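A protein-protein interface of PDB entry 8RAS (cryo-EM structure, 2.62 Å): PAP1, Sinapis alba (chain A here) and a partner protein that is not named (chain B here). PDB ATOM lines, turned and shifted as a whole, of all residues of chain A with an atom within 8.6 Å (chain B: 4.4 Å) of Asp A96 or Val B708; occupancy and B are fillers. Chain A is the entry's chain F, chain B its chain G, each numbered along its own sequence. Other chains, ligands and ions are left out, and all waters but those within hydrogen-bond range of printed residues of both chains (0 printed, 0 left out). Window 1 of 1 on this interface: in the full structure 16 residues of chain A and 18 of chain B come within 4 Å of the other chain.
The side-chain carboxylate (OD2) of Asp A96 is in hydrogen-bond range of the side-chain amide nitrogen (ND2) of Asn B705 (3.1 Å). The side-chain carboxylate of Asp A96 lies within salt-bridge range of the guanidinium group of Arg B703, 2.8 Å away.
Of the 10 printed residues of chain B, 6 touch a printed residue of chain A. Hydrophobic or aromatic side chains of chain A that line the printed part of chain B: Phe A74, Tyr A95 and Ala A100.
Of the printed residues of chain B, Glu A77 touches Leu B707 (3.8 Å). Of the printed residues of chain B, Glu A92 touches Arg B703. Asp A96 touches three residues of chain B. Printed residues of chain A within 4 Å of Arg B703: Glu A92, Tyr A95 and Asp A96. Of chain A, only Phe A74, Asp A96 and Ala A100 come within 4 Å of Val B708. Printed residues of chain A within 4 Å of Leu B745: Ala A100. The nearest residue of chain A that does not touch Val B708 is Ala A99 (4.3 Å). The nearest printed residue of chain B that does not touch Tyr A95 is Val B708 (6.2 Å).
Among the printed residues, merely in contact across the chains: Phe A74 with Val B708, Phe A74 with Leu B707, Ala A100 with Leu B745, Ala A99 with Val B747, Glu A92 with Arg B703, Tyr A95 with Arg B703, Glu A77 with Leu B707, Asp A96 with Val B708 and Ala A100 with Val B708.
O of Leu B745 is in hydrogen-bond range of N of Trp B709 (2.9 Å). The backbone carbonyl oxygen (O) of Arg B703 lies within hydrogen-bond range of the backbone NH (N) of Ser B710 (3.1 Å). The side-chain carboxylate (OE1) of Glu A77 lies within salt-bridge range of the guanidinium group (NE) of Arg A81 (2.8 Å). The guanidinium group (NH1) of Arg A81 is in salt-bridge range of the side-chain carboxylate (OE1) of Glu A92, at 3.5 Å. O of Asn B705 lies close to NE1 of Trp B709 (3.3 Å). N of Leu B707 sits at hydrogen-bond distance from OD1 of Asn B705 (3.0 Å).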
ATOM      1  N   LEU A  70      22.256  11.197   1.496  1.00  0.00           N
ATOM      2  CA  LEU A  70      20.993  11.633   0.908  1.00  0.00           C
ATOM      3  C   LEU A  70      20.780  13.126   1.119  1.00  0.00           C
ATOM      4  O   LEU A  70      20.388  13.844   0.190  1.00  0.00           O
ATOM      5  CB  LEU A  70      19.833  10.835   1.503  1.00  0.00           C
ATOM      6  CG  LEU A  70      19.396   9.584   0.741  1.00  0.00           C
ATOM      7  CD1 LEU A  70      18.199   8.939   1.418  1.00  0.00           C
ATOM      8  CD2 LEU A  70      19.084   9.917  -0.710  1.00  0.00           C
ATOM      9  N   PHE A  74      20.515  15.990  -1.816  1.00  0.00           N
ATOM     10  CA  PHE A  74      19.318  16.817  -1.898  1.00  0.00           C
ATOM     11  C   PHE A  74      19.652  18.288  -1.685  1.00  0.00           C
ATOM     12  O   PHE A  74      19.124  19.156  -2.388  1.00  0.00           O
ATOM     13  CB  PHE A  74      18.290  16.337  -0.878  1.00  0.00           C
ATOM     14  CG  PHE A  74      17.327  15.327  -1.428  1.00  0.00           C
ATOM     15  CD1 PHE A  74      15.969  15.452  -1.213  1.00  0.00           C
ATOM     16  CD2 PHE A  74      17.786  14.239  -2.149  1.00  0.00           C
ATOM     17  CE1 PHE A  74      15.083  14.521  -1.713  1.00  0.00           C
ATOM     18  CE2 PHE A  74      16.907  13.303  -2.651  1.00  0.00           C
ATOM     19  CZ  PHE A  74      15.554  13.446  -2.433  1.00  0.00           C
ATOM     20  N   GLU A  77      21.357  19.642  -4.881  1.00  0.00           N
ATOM     21  CA  GLU A  77      20.433  19.889  -5.983  1.00  0.00           C
ATOM     22  C   GLU A  77      19.526  21.079  -5.670  1.00  0.00           C
ATOM     23  O   GLU A  77      19.226  21.891  -6.556  1.00  0.00           O
ATOM     24  CB  GLU A  77      19.631  18.619  -6.271  1.00  0.00           C
ATOM     25  CG  GLU A  77      19.104  18.472  -7.695  1.00  0.00           C
ATOM     26  CD  GLU A  77      17.944  19.376  -8.017  1.00  0.00           C
ATOM     27  OE1 GLU A  77      16.937  19.331  -7.288  1.00  0.00           O
ATOM     28  OE2 GLU A  77      18.029  20.109  -9.020  1.00  0.00           O
ATOM     29  N   LEU A  78      19.105  21.216  -4.407  1.00  0.00           N
ATOM     30  CA  LEU A  78      18.283  22.353  -3.998  1.00  0.00           C
ATOM     31  C   LEU A  78      19.041  23.669  -4.116  1.00  0.00           C
ATOM     32  O   LEU A  78      18.488  24.665  -4.594  1.00  0.00           O
ATOM     33  CB  LEU A  78      17.799  22.153  -2.562  1.00  0.00           C
ATOM     34  CG  LEU A  78      16.858  23.214  -1.990  1.00  0.00           C
ATOM     35  CD1 LEU A  78      15.741  22.566  -1.190  1.00  0.00           C
ATOM     36  CD2 LEU A  78      17.618  24.213  -1.133  1.00  0.00           C
ATOM     37  N   ARG A  81      19.157  24.583  -7.738  1.00  0.00           N
ATOM     38  CA  ARG A  81      17.907  25.177  -8.213  1.00  0.00           C
ATOM     39  C   ARG A  81      17.711  26.587  -7.674  1.00  0.00           C
ATOM     40  O   ARG A  81      17.139  27.441  -8.362  1.00  0.00           O
ATOM     41  CB  ARG A  81      16.716  24.302  -7.831  1.00  0.00           C
ATOM     42  CG  ARG A  81      16.864  22.861  -8.243  1.00  0.00           C
ATOM     43  CD  ARG A  81      15.695  22.404  -9.092  1.00  0.00           C
ATOM     44  NE  ARG A  81      15.297  21.036  -8.789  1.00  0.00           N
ATOM     45  CZ  ARG A  81      14.308  20.397  -9.398  1.00  0.00           C
ATOM     46  NH1 ARG A  81      13.599  20.975 -10.353  1.00  0.00           N
ATOM     47  NH2 ARG A  81      14.026  19.147  -9.042  1.00  0.00           N
ATOM     48  N   GLY A  89      11.396  24.998  -8.420  1.00  0.00           N
ATOM     49  CA  GLY A  89      12.235  23.816  -8.312  1.00  0.00           C
ATOM     50  C   GLY A  89      12.676  23.545  -6.888  1.00  0.00           C
ATOM     51  O   GLY A  89      12.757  22.390  -6.460  1.00  0.00           O
ATOM     52  N   VAL A  90      12.963  24.605  -6.131  1.00  0.00           N
ATOM     53  CA  VAL A  90      13.303  24.436  -4.722  1.00  0.00           C
ATOM     54  C   VAL A  90      12.120  23.852  -3.961  1.00  0.00           C
ATOM     55  O   VAL A  90      12.292  23.033  -3.049  1.00  0.00           O
ATOM     56  CB  VAL A  90      13.766  25.771  -4.117  1.00  0.00           C
ATOM     57  CG1 VAL A  90      14.220  25.562  -2.690  1.00  0.00           C
ATOM     58  CG2 VAL A  90      14.888  26.366  -4.949  1.00  0.00           C
ATOM     59  N   SER A  91      10.902  24.263  -4.319  1.00  0.00           N
ATOM     60  CA  SER A  91       9.720  23.672  -3.696  1.00  0.00           C
ATOM     61  C   SER A  91       9.599  22.190  -4.034  1.00  0.00           C
ATOM     62  O   SER A  91       9.231  21.378  -3.175  1.00  0.00           O
ATOM     63  CB  SER A  91       8.464  24.428  -4.123  1.00  0.00           C
ATOM     64  OG  SER A  91       7.364  24.083  -3.300  1.00  0.00           O
ATOM     65  N   GLU A  92       9.892  21.819  -5.285  1.00  0.00           N
ATOM     66  CA  GLU A  92       9.901  20.398  -5.633  1.00  0.00           C
ATOM     67  C   GLU A  92      10.924  19.637  -4.801  1.00  0.00           C
ATOM     68  O   GLU A  92      10.648  18.530  -4.328  1.00  0.00           O
ATOM     69  CB  GLU A  92      10.179  20.174  -7.123  1.00  0.00           C
ATOM     70  CG  GLU A  92       9.804  21.295  -8.055  1.00  0.00           C
ATOM     71  CD  GLU A  92      10.085  20.966  -9.510  1.00  0.00           C
ATOM     72  OE1 GLU A  92      10.383  19.791  -9.810  1.00  0.00           O
ATOM     73  OE2 GLU A  92      10.021  21.885 -10.352  1.00  0.00           O
ATOM     74  N   VAL A  93      12.113  20.212  -4.612  1.00  0.00           N
ATOM     75  CA  VAL A  93      13.132  19.535  -3.814  1.00  0.00           C
ATOM     76  C   VAL A  93      12.678  19.398  -2.366  1.00  0.00           C
ATOM     77  O   VAL A  93      12.919  18.373  -1.721  1.00  0.00           O
ATOM     78  CB  VAL A  93      14.480  20.269  -3.907  1.00  0.00           C
ATOM     79  CG1 VAL A  93      15.556  19.467  -3.196  1.00  0.00           C
ATOM     80  CG2 VAL A  93      14.861  20.487  -5.346  1.00  0.00           C
ATOM     81  N   ILE A  94      12.024  20.430  -1.828  1.00  0.00           N
ATOM     82  CA  ILE A  94      11.556  20.372  -0.444  1.00  0.00           C
ATOM     83  C   ILE A  94      10.499  19.287  -0.284  1.00  0.00           C
ATOM     84  O   ILE A  94      10.509  18.523   0.690  1.00  0.00           O
ATOM     85  CB  ILE A  94      11.037  21.750   0.002  1.00  0.00           C
ATOM     86  CG1 ILE A  94      12.210  22.655   0.378  1.00  0.00           C
ATOM     87  CG2 ILE A  94      10.081  21.616   1.176  1.00  0.00           C
ATOM     88  CD1 ILE A  94      11.795  24.036   0.824  1.00  0.00           C
ATOM     89  N   TYR A  95       9.572  19.195  -1.241  1.00  0.00           N
ATOM     90  CA  TYR A  95       8.577  18.129  -1.181  1.00  0.00           C
ATOM     91  C   TYR A  95       9.212  16.757  -1.371  1.00  0.00           C
ATOM     92  O   TYR A  95       8.742  15.771  -0.789  1.00  0.00           O
ATOM     93  CB  TYR A  95       7.484  18.374  -2.218  1.00  0.00           C
ATOM     94  CG  TYR A  95       6.494  19.430  -1.788  1.00  0.00           C
ATOM     95  CD1 TYR A  95       6.118  19.549  -0.457  1.00  0.00           C
ATOM     96  CD2 TYR A  95       5.942  20.311  -2.706  1.00  0.00           C
ATOM     97  CE1 TYR A  95       5.216  20.512  -0.053  1.00  0.00           C
ATOM     98  CE2 TYR A  95       5.039  21.279  -2.311  1.00  0.00           C
ATOM     99  CZ  TYR A  95       4.680  21.375  -0.983  1.00  0.00           C
ATOM    100  OH  TYR A  95       3.781  22.336  -0.585  1.00  0.00           O
ATOM    101  N   ASP A  96      10.283  16.673  -2.162  1.00  0.00           N
ATOM    102  CA  ASP A  96      11.025  15.420  -2.269  1.00  0.00           C
ATOM    103  C   ASP A  96      11.646  15.037  -0.932  1.00  0.00           C
ATOM    104  O   ASP A  96      11.645  13.860  -0.556  1.00  0.00           O
ATOM    105  CB  ASP A  96      12.102  15.533  -3.347  1.00  0.00           C
ATOM    106  CG  ASP A  96      11.521  15.688  -4.737  1.00  0.00           C
ATOM    107  OD1 ASP A  96      10.280  15.687  -4.865  1.00  0.00           O
ATOM    108  OD2 ASP A  96      12.307  15.813  -5.700  1.00  0.00           O
ATOM    109  N   MET A  97      12.191  16.015  -0.207  1.00  0.00           N
ATOM    110  CA  MET A  97      12.719  15.736   1.126  1.00  0.00           C
ATOM    111  C   MET A  97      11.612  15.275   2.063  1.00  0.00           C
ATOM    112  O   MET A  97      11.810  14.364   2.876  1.00  0.00           O
ATOM    113  CB  MET A  97      13.418  16.966   1.705  1.00  0.00           C
ATOM    114  CG  MET A  97      14.450  17.601   0.795  1.00  0.00           C
ATOM    115  SD  MET A  97      15.496  18.829   1.595  1.00  0.00           S
ATOM    116  CE  MET A  97      14.980  18.649   3.295  1.00  0.00           C
ATOM    117  N   ILE A  98      10.440  15.905   1.968  1.00  0.00           N
ATOM    118  CA  ILE A  98       9.308  15.515   2.807  1.00  0.00           C
ATOM    119  C   ILE A  98       8.914  14.070   2.527  1.00  0.00           C
ATOM    120  O   ILE A  98       8.684  13.279   3.448  1.00  0.00           O
ATOM    121  CB  ILE A  98       8.125  16.477   2.594  1.00  0.00           C
ATOM    122  CG1 ILE A  98       8.321  17.751   3.416  1.00  0.00           C
ATOM    123  CG2 ILE A  98       6.809  15.808   2.961  1.00  0.00           C
ATOM    124  CD1 ILE A  98       8.619  17.492   4.876  1.00  0.00           C
ATOM    125  N   ALA A  99       8.837  13.705   1.245  1.00  0.00           N
ATOM    126  CA  ALA A  99       8.502  12.330   0.884  1.00  0.00           C
ATOM    127  C   ALA A  99       9.580  11.357   1.348  1.00  0.00           C
ATOM    128  O   ALA A  99       9.273  10.256   1.821  1.00  0.00           O
ATOM    129  CB  ALA A  99       8.293  12.220  -0.625  1.00  0.00           C
ATOM    130  N   ALA A 100      10.849  11.746   1.223  1.00  0.00           N
ATOM    131  CA  ALA A 100      11.965  10.890   1.597  1.00  0.00           C
ATOM    132  C   ALA A 100      12.126  10.741   3.103  1.00  0.00           C
ATOM    133  O   ALA A 100      12.918   9.900   3.542  1.00  0.00           O
ATOM    134  CB  ALA A 100      13.262  11.438   0.998  1.00  0.00           C
ATOM    135  N   GLY A 101      11.403  11.523   3.898  1.00  0.00           N
ATOM    136  CA  GLY A 101      11.546  11.493   5.335  1.00  0.00           C
ATOM    137  C   GLY A 101      12.561  12.462   5.897  1.00  0.00           C
ATOM    138  O   GLY A 101      12.682  12.563   7.125  1.00  0.00           O
ATOM    139  N   LEU A 102      13.291  13.177   5.046  1.00  0.00           N
ATOM    140  CA  LEU A 102      14.272  14.147   5.511  1.00  0.00           C
ATOM    141  C   LEU A 102      13.557  15.411   5.969  1.00  0.00           C
ATOM    142  O   LEU A 102      12.799  16.016   5.202  1.00  0.00           O
ATOM    143  CB  LEU A 102      15.274  14.464   4.402  1.00  0.00           C
ATOM    144  CG  LEU A 102      15.899  13.259   3.694  1.00  0.00           C
ATOM    145  CD1 LEU A 102      16.606  13.691   2.419  1.00  0.00           C
ATOM    146  CD2 LEU A 102      16.858  12.533   4.622  1.00  0.00           C
ATOM    147  N   SER A 103      13.793  15.808   7.211  1.00  0.00           N
ATOM    148  CA  SER A 103      13.155  17.005   7.743  1.00  0.00           C
ATOM    149  C   SER A 103      13.789  18.246   7.126  1.00  0.00           C
ATOM    150  O   SER A 103      15.019  18.366   7.112  1.00  0.00           O
ATOM    151  CB  SER A 103      13.279  17.047   9.263  1.00  0.00           C
ATOM    152  OG  SER A 103      12.455  16.065   9.868  1.00  0.00           O
ATOM    153  N   PRO A 104      12.995  19.183   6.606  1.00  0.00           N
ATOM    154  CA  PRO A 104      13.579  20.388   6.003  1.00  0.00           C
ATOM    155  C   PRO A 104      14.186  21.319   7.038  1.00  0.00           C
ATOM    156  O   PRO A 104      13.467  21.965   7.808  1.00  0.00           O
ATOM    157  CB  PRO A 104      12.386  21.041   5.288  1.00  0.00           C
ATOM    158  CG  PRO A 104      11.315  19.991   5.249  1.00  0.00           C
ATOM    159  CD  PRO A 104      11.534  19.146   6.456  1.00  0.00           C
ATOM    160  N   ARG B 703       5.190  10.595  -7.521  1.00  0.00           N
ATOM    161  CA  ARG B 703       6.216  11.597  -7.778  1.00  0.00           C
ATOM    162  C   ARG B 703       7.369  10.925  -8.506  1.00  0.00           C
ATOM    163  O   ARG B 703       7.889   9.907  -8.041  1.00  0.00           O
ATOM    164  CB  ARG B 703       6.711  12.240  -6.479  1.00  0.00           C
ATOM    165  CG  ARG B 703       5.618  12.850  -5.621  1.00  0.00           C
ATOM    166  CD  ARG B 703       6.206  13.591  -4.431  1.00  0.00           C
ATOM    167  NE  ARG B 703       7.153  14.620  -4.843  1.00  0.00           N
ATOM    168  CZ  ARG B 703       6.825  15.877  -5.108  1.00  0.00           C
ATOM    169  NH1 ARG B 703       5.575  16.300  -5.010  1.00  0.00           N
ATOM    170  NH2 ARG B 703       7.774  16.731  -5.480  1.00  0.00           N
ATOM    171  N   LYS B 704       7.768  11.492  -9.644  1.00  0.00           N
ATOM    172  CA  LYS B 704       8.831  10.928 -10.466  1.00  0.00           C
ATOM    173  C   LYS B 704       9.863  12.007 -10.752  1.00  0.00           C
ATOM    174  O   LYS B 704       9.539  13.031 -11.361  1.00  0.00           O
ATOM    175  CB  LYS B 704       8.277  10.358 -11.775  1.00  0.00           C
ATOM    176  CG  LYS B 704       7.056   9.468 -11.606  1.00  0.00           C
ATOM    177  CD  LYS B 704       7.439   8.093 -11.092  1.00  0.00           C
ATOM    178  CE  LYS B 704       6.243   7.157 -11.077  1.00  0.00           C
ATOM    179  NZ  LYS B 704       5.737   6.881 -12.450  1.00  0.00           N
ATOM    180  N   ASN B 705      11.098  11.773 -10.319  1.00  0.00           N
ATOM    181  CA  ASN B 705      12.203  12.684 -10.585  1.00  0.00           C
ATOM    182  C   ASN B 705      13.506  11.924 -10.369  1.00  0.00           C
ATOM    183  O   ASN B 705      13.510  10.765  -9.948  1.00  0.00           O
ATOM    184  CB  ASN B 705      12.127  13.932  -9.701  1.00  0.00           C
ATOM    185  CG  ASN B 705      11.848  13.605  -8.250  1.00  0.00           C
ATOM    186  OD1 ASN B 705      12.642  12.936  -7.589  1.00  0.00           O
ATOM    187  ND2 ASN B 705      10.714  14.075  -7.745  1.00  0.00           N
ATOM    188  N   LYS B 706      14.622  12.596 -10.661  1.00  0.00           N
ATOM    189  CA  LYS B 706      15.934  11.976 -10.515  1.00  0.00           C
ATOM    190  C   LYS B 706      16.260  11.648  -9.064  1.00  0.00           C
ATOM    191  O   LYS B 706      17.149  10.828  -8.807  1.00  0.00           O
ATOM    192  CB  LYS B 706      17.006  12.898 -11.106  1.00  0.00           C
ATOM    193  CG  LYS B 706      18.407  12.302 -11.173  1.00  0.00           C
ATOM    194  CD  LYS B 706      18.894  12.196 -12.606  1.00  0.00           C
ATOM    195  CE  LYS B 706      18.829  13.540 -13.312  1.00  0.00           C
ATOM    196  NZ  LYS B 706      18.744  13.388 -14.790  1.00  0.00           N
ATOM    197  N   LEU B 707      15.552  12.249  -8.110  1.00  0.00           N
ATOM    198  CA  LEU B 707      15.857  12.082  -6.693  1.00  0.00           C
ATOM    199  C   LEU B 707      14.961  11.047  -6.020  1.00  0.00           C
ATOM    200  O   LEU B 707      15.457  10.074  -5.445  1.00  0.00           O
ATOM    201  CB  LEU B 707      15.739  13.434  -5.976  1.00  0.00           C
ATOM    202  CG  LEU B 707      16.742  14.511  -6.390  1.00  0.00           C
ATOM    203  CD1 LEU B 707      16.365  15.852  -5.784  1.00  0.00           C
ATOM    204  CD2 LEU B 707      18.155  14.112  -5.990  1.00  0.00           C
ATOM    205  N   VAL B 708      13.645  11.237  -6.082  1.00  0.00           N
ATOM    206  CA  VAL B 708      12.700  10.427  -5.323  1.00  0.00           C
ATOM    207  C   VAL B 708      11.619   9.903  -6.258  1.00  0.00           C
ATOM    208  O   VAL B 708      11.031  10.670  -7.028  1.00  0.00           O
ATOM    209  CB  VAL B 708      12.077  11.227  -4.161  1.00  0.00           C
ATOM    210  CG1 VAL B 708      10.672  10.740  -3.858  1.00  0.00           C
ATOM    211  CG2 VAL B 708      12.948  11.122  -2.924  1.00  0.00           C
ATOM    212  N   TRP B 709      11.371   8.597  -6.195  1.00  0.00           N
ATOM    213  CA  TRP B 709      10.216   7.961  -6.826  1.00  0.00           C
ATOM    214  C   TRP B 709       9.313   7.494  -5.690  1.00  0.00           C
ATOM    215  O   TRP B 709       9.606   6.497  -5.025  1.00  0.00           O
ATOM    216  CB  TRP B 709      10.643   6.803  -7.722  1.00  0.00           C
ATOM    217  CG  TRP B 709      10.875   7.194  -9.147  1.00  0.00           C
ATOM    218  CD1 TRP B 709      11.514   8.312  -9.595  1.00  0.00           C
ATOM    219  CD2 TRP B 709      10.475   6.466 -10.314  1.00  0.00           C
ATOM    220  NE1 TRP B 709      11.534   8.327 -10.968  1.00  0.00           N
ATOM    221  CE2 TRP B 709      10.902   7.204 -11.433  1.00  0.00           C
ATOM    222  CE3 TRP B 709       9.794   5.264 -10.519  1.00  0.00           C
ATOM    223  CZ2 TRP B 709      10.672   6.779 -12.740  1.00  0.00           C
ATOM    224  CZ3 TRP B 709       9.568   4.842 -11.815  1.00  0.00           C
ATOM    225  CH2 TRP B 709      10.005   5.598 -12.908  1.00  0.00           C
ATOM    226  N   SER B 710       8.216   8.211  -5.464  1.00  0.00           N
ATOM    227  CA  SER B 710       7.409   8.022  -4.270  1.00  0.00           C
ATOM    228  C   SER B 710       5.982   7.624  -4.621  1.00  0.00           C
ATOM    229  O   SER B 710       5.467   7.957  -5.691  1.00  0.00           O
ATOM    230  CB  SER B 710       7.379   9.294  -3.417  1.00  0.00           C
ATOM    231  OG  SER B 710       6.402  10.201  -3.892  1.00  0.00           O
ATOM    232  N   LEU B 745      16.365   7.224  -4.835  1.00  0.00           N
ATOM    233  CA  LEU B 745      15.580   6.616  -3.773  1.00  0.00           C
ATOM    234  C   LEU B 745      14.155   6.387  -4.256  1.00  0.00           C
ATOM    235  O   LEU B 745      13.554   7.267  -4.875  1.00  0.00           O
ATOM    236  CB  LEU B 745      15.590   7.505  -2.523  1.00  0.00           C
ATOM    237  CG  LEU B 745      14.415   7.450  -1.546  1.00  0.00           C
ATOM    238  CD1 LEU B 745      14.258   6.077  -0.935  1.00  0.00           C
ATOM    239  CD2 LEU B 745      14.612   8.487  -0.464  1.00  0.00           C
ATOM    240  N   VAL B 747      10.612   5.498  -2.403  1.00  0.00           N
ATOM    241  CA  VAL B 747      10.098   5.568  -1.043  1.00  0.00           C
ATOM    242  C   VAL B 747       8.584   5.397  -1.071  1.00  0.00           C
ATOM    243  O   VAL B 747       7.925   5.624  -2.087  1.00  0.00           O
ATOM    244  CB  VAL B 747      10.491   6.899  -0.356  1.00  0.00           C
ATOM    245  CG1 VAL B 747       9.720   8.064  -0.956  1.00  0.00           C
ATOM    246  CG2 VAL B 747      10.308   6.827   1.157  1.00  0.00           C
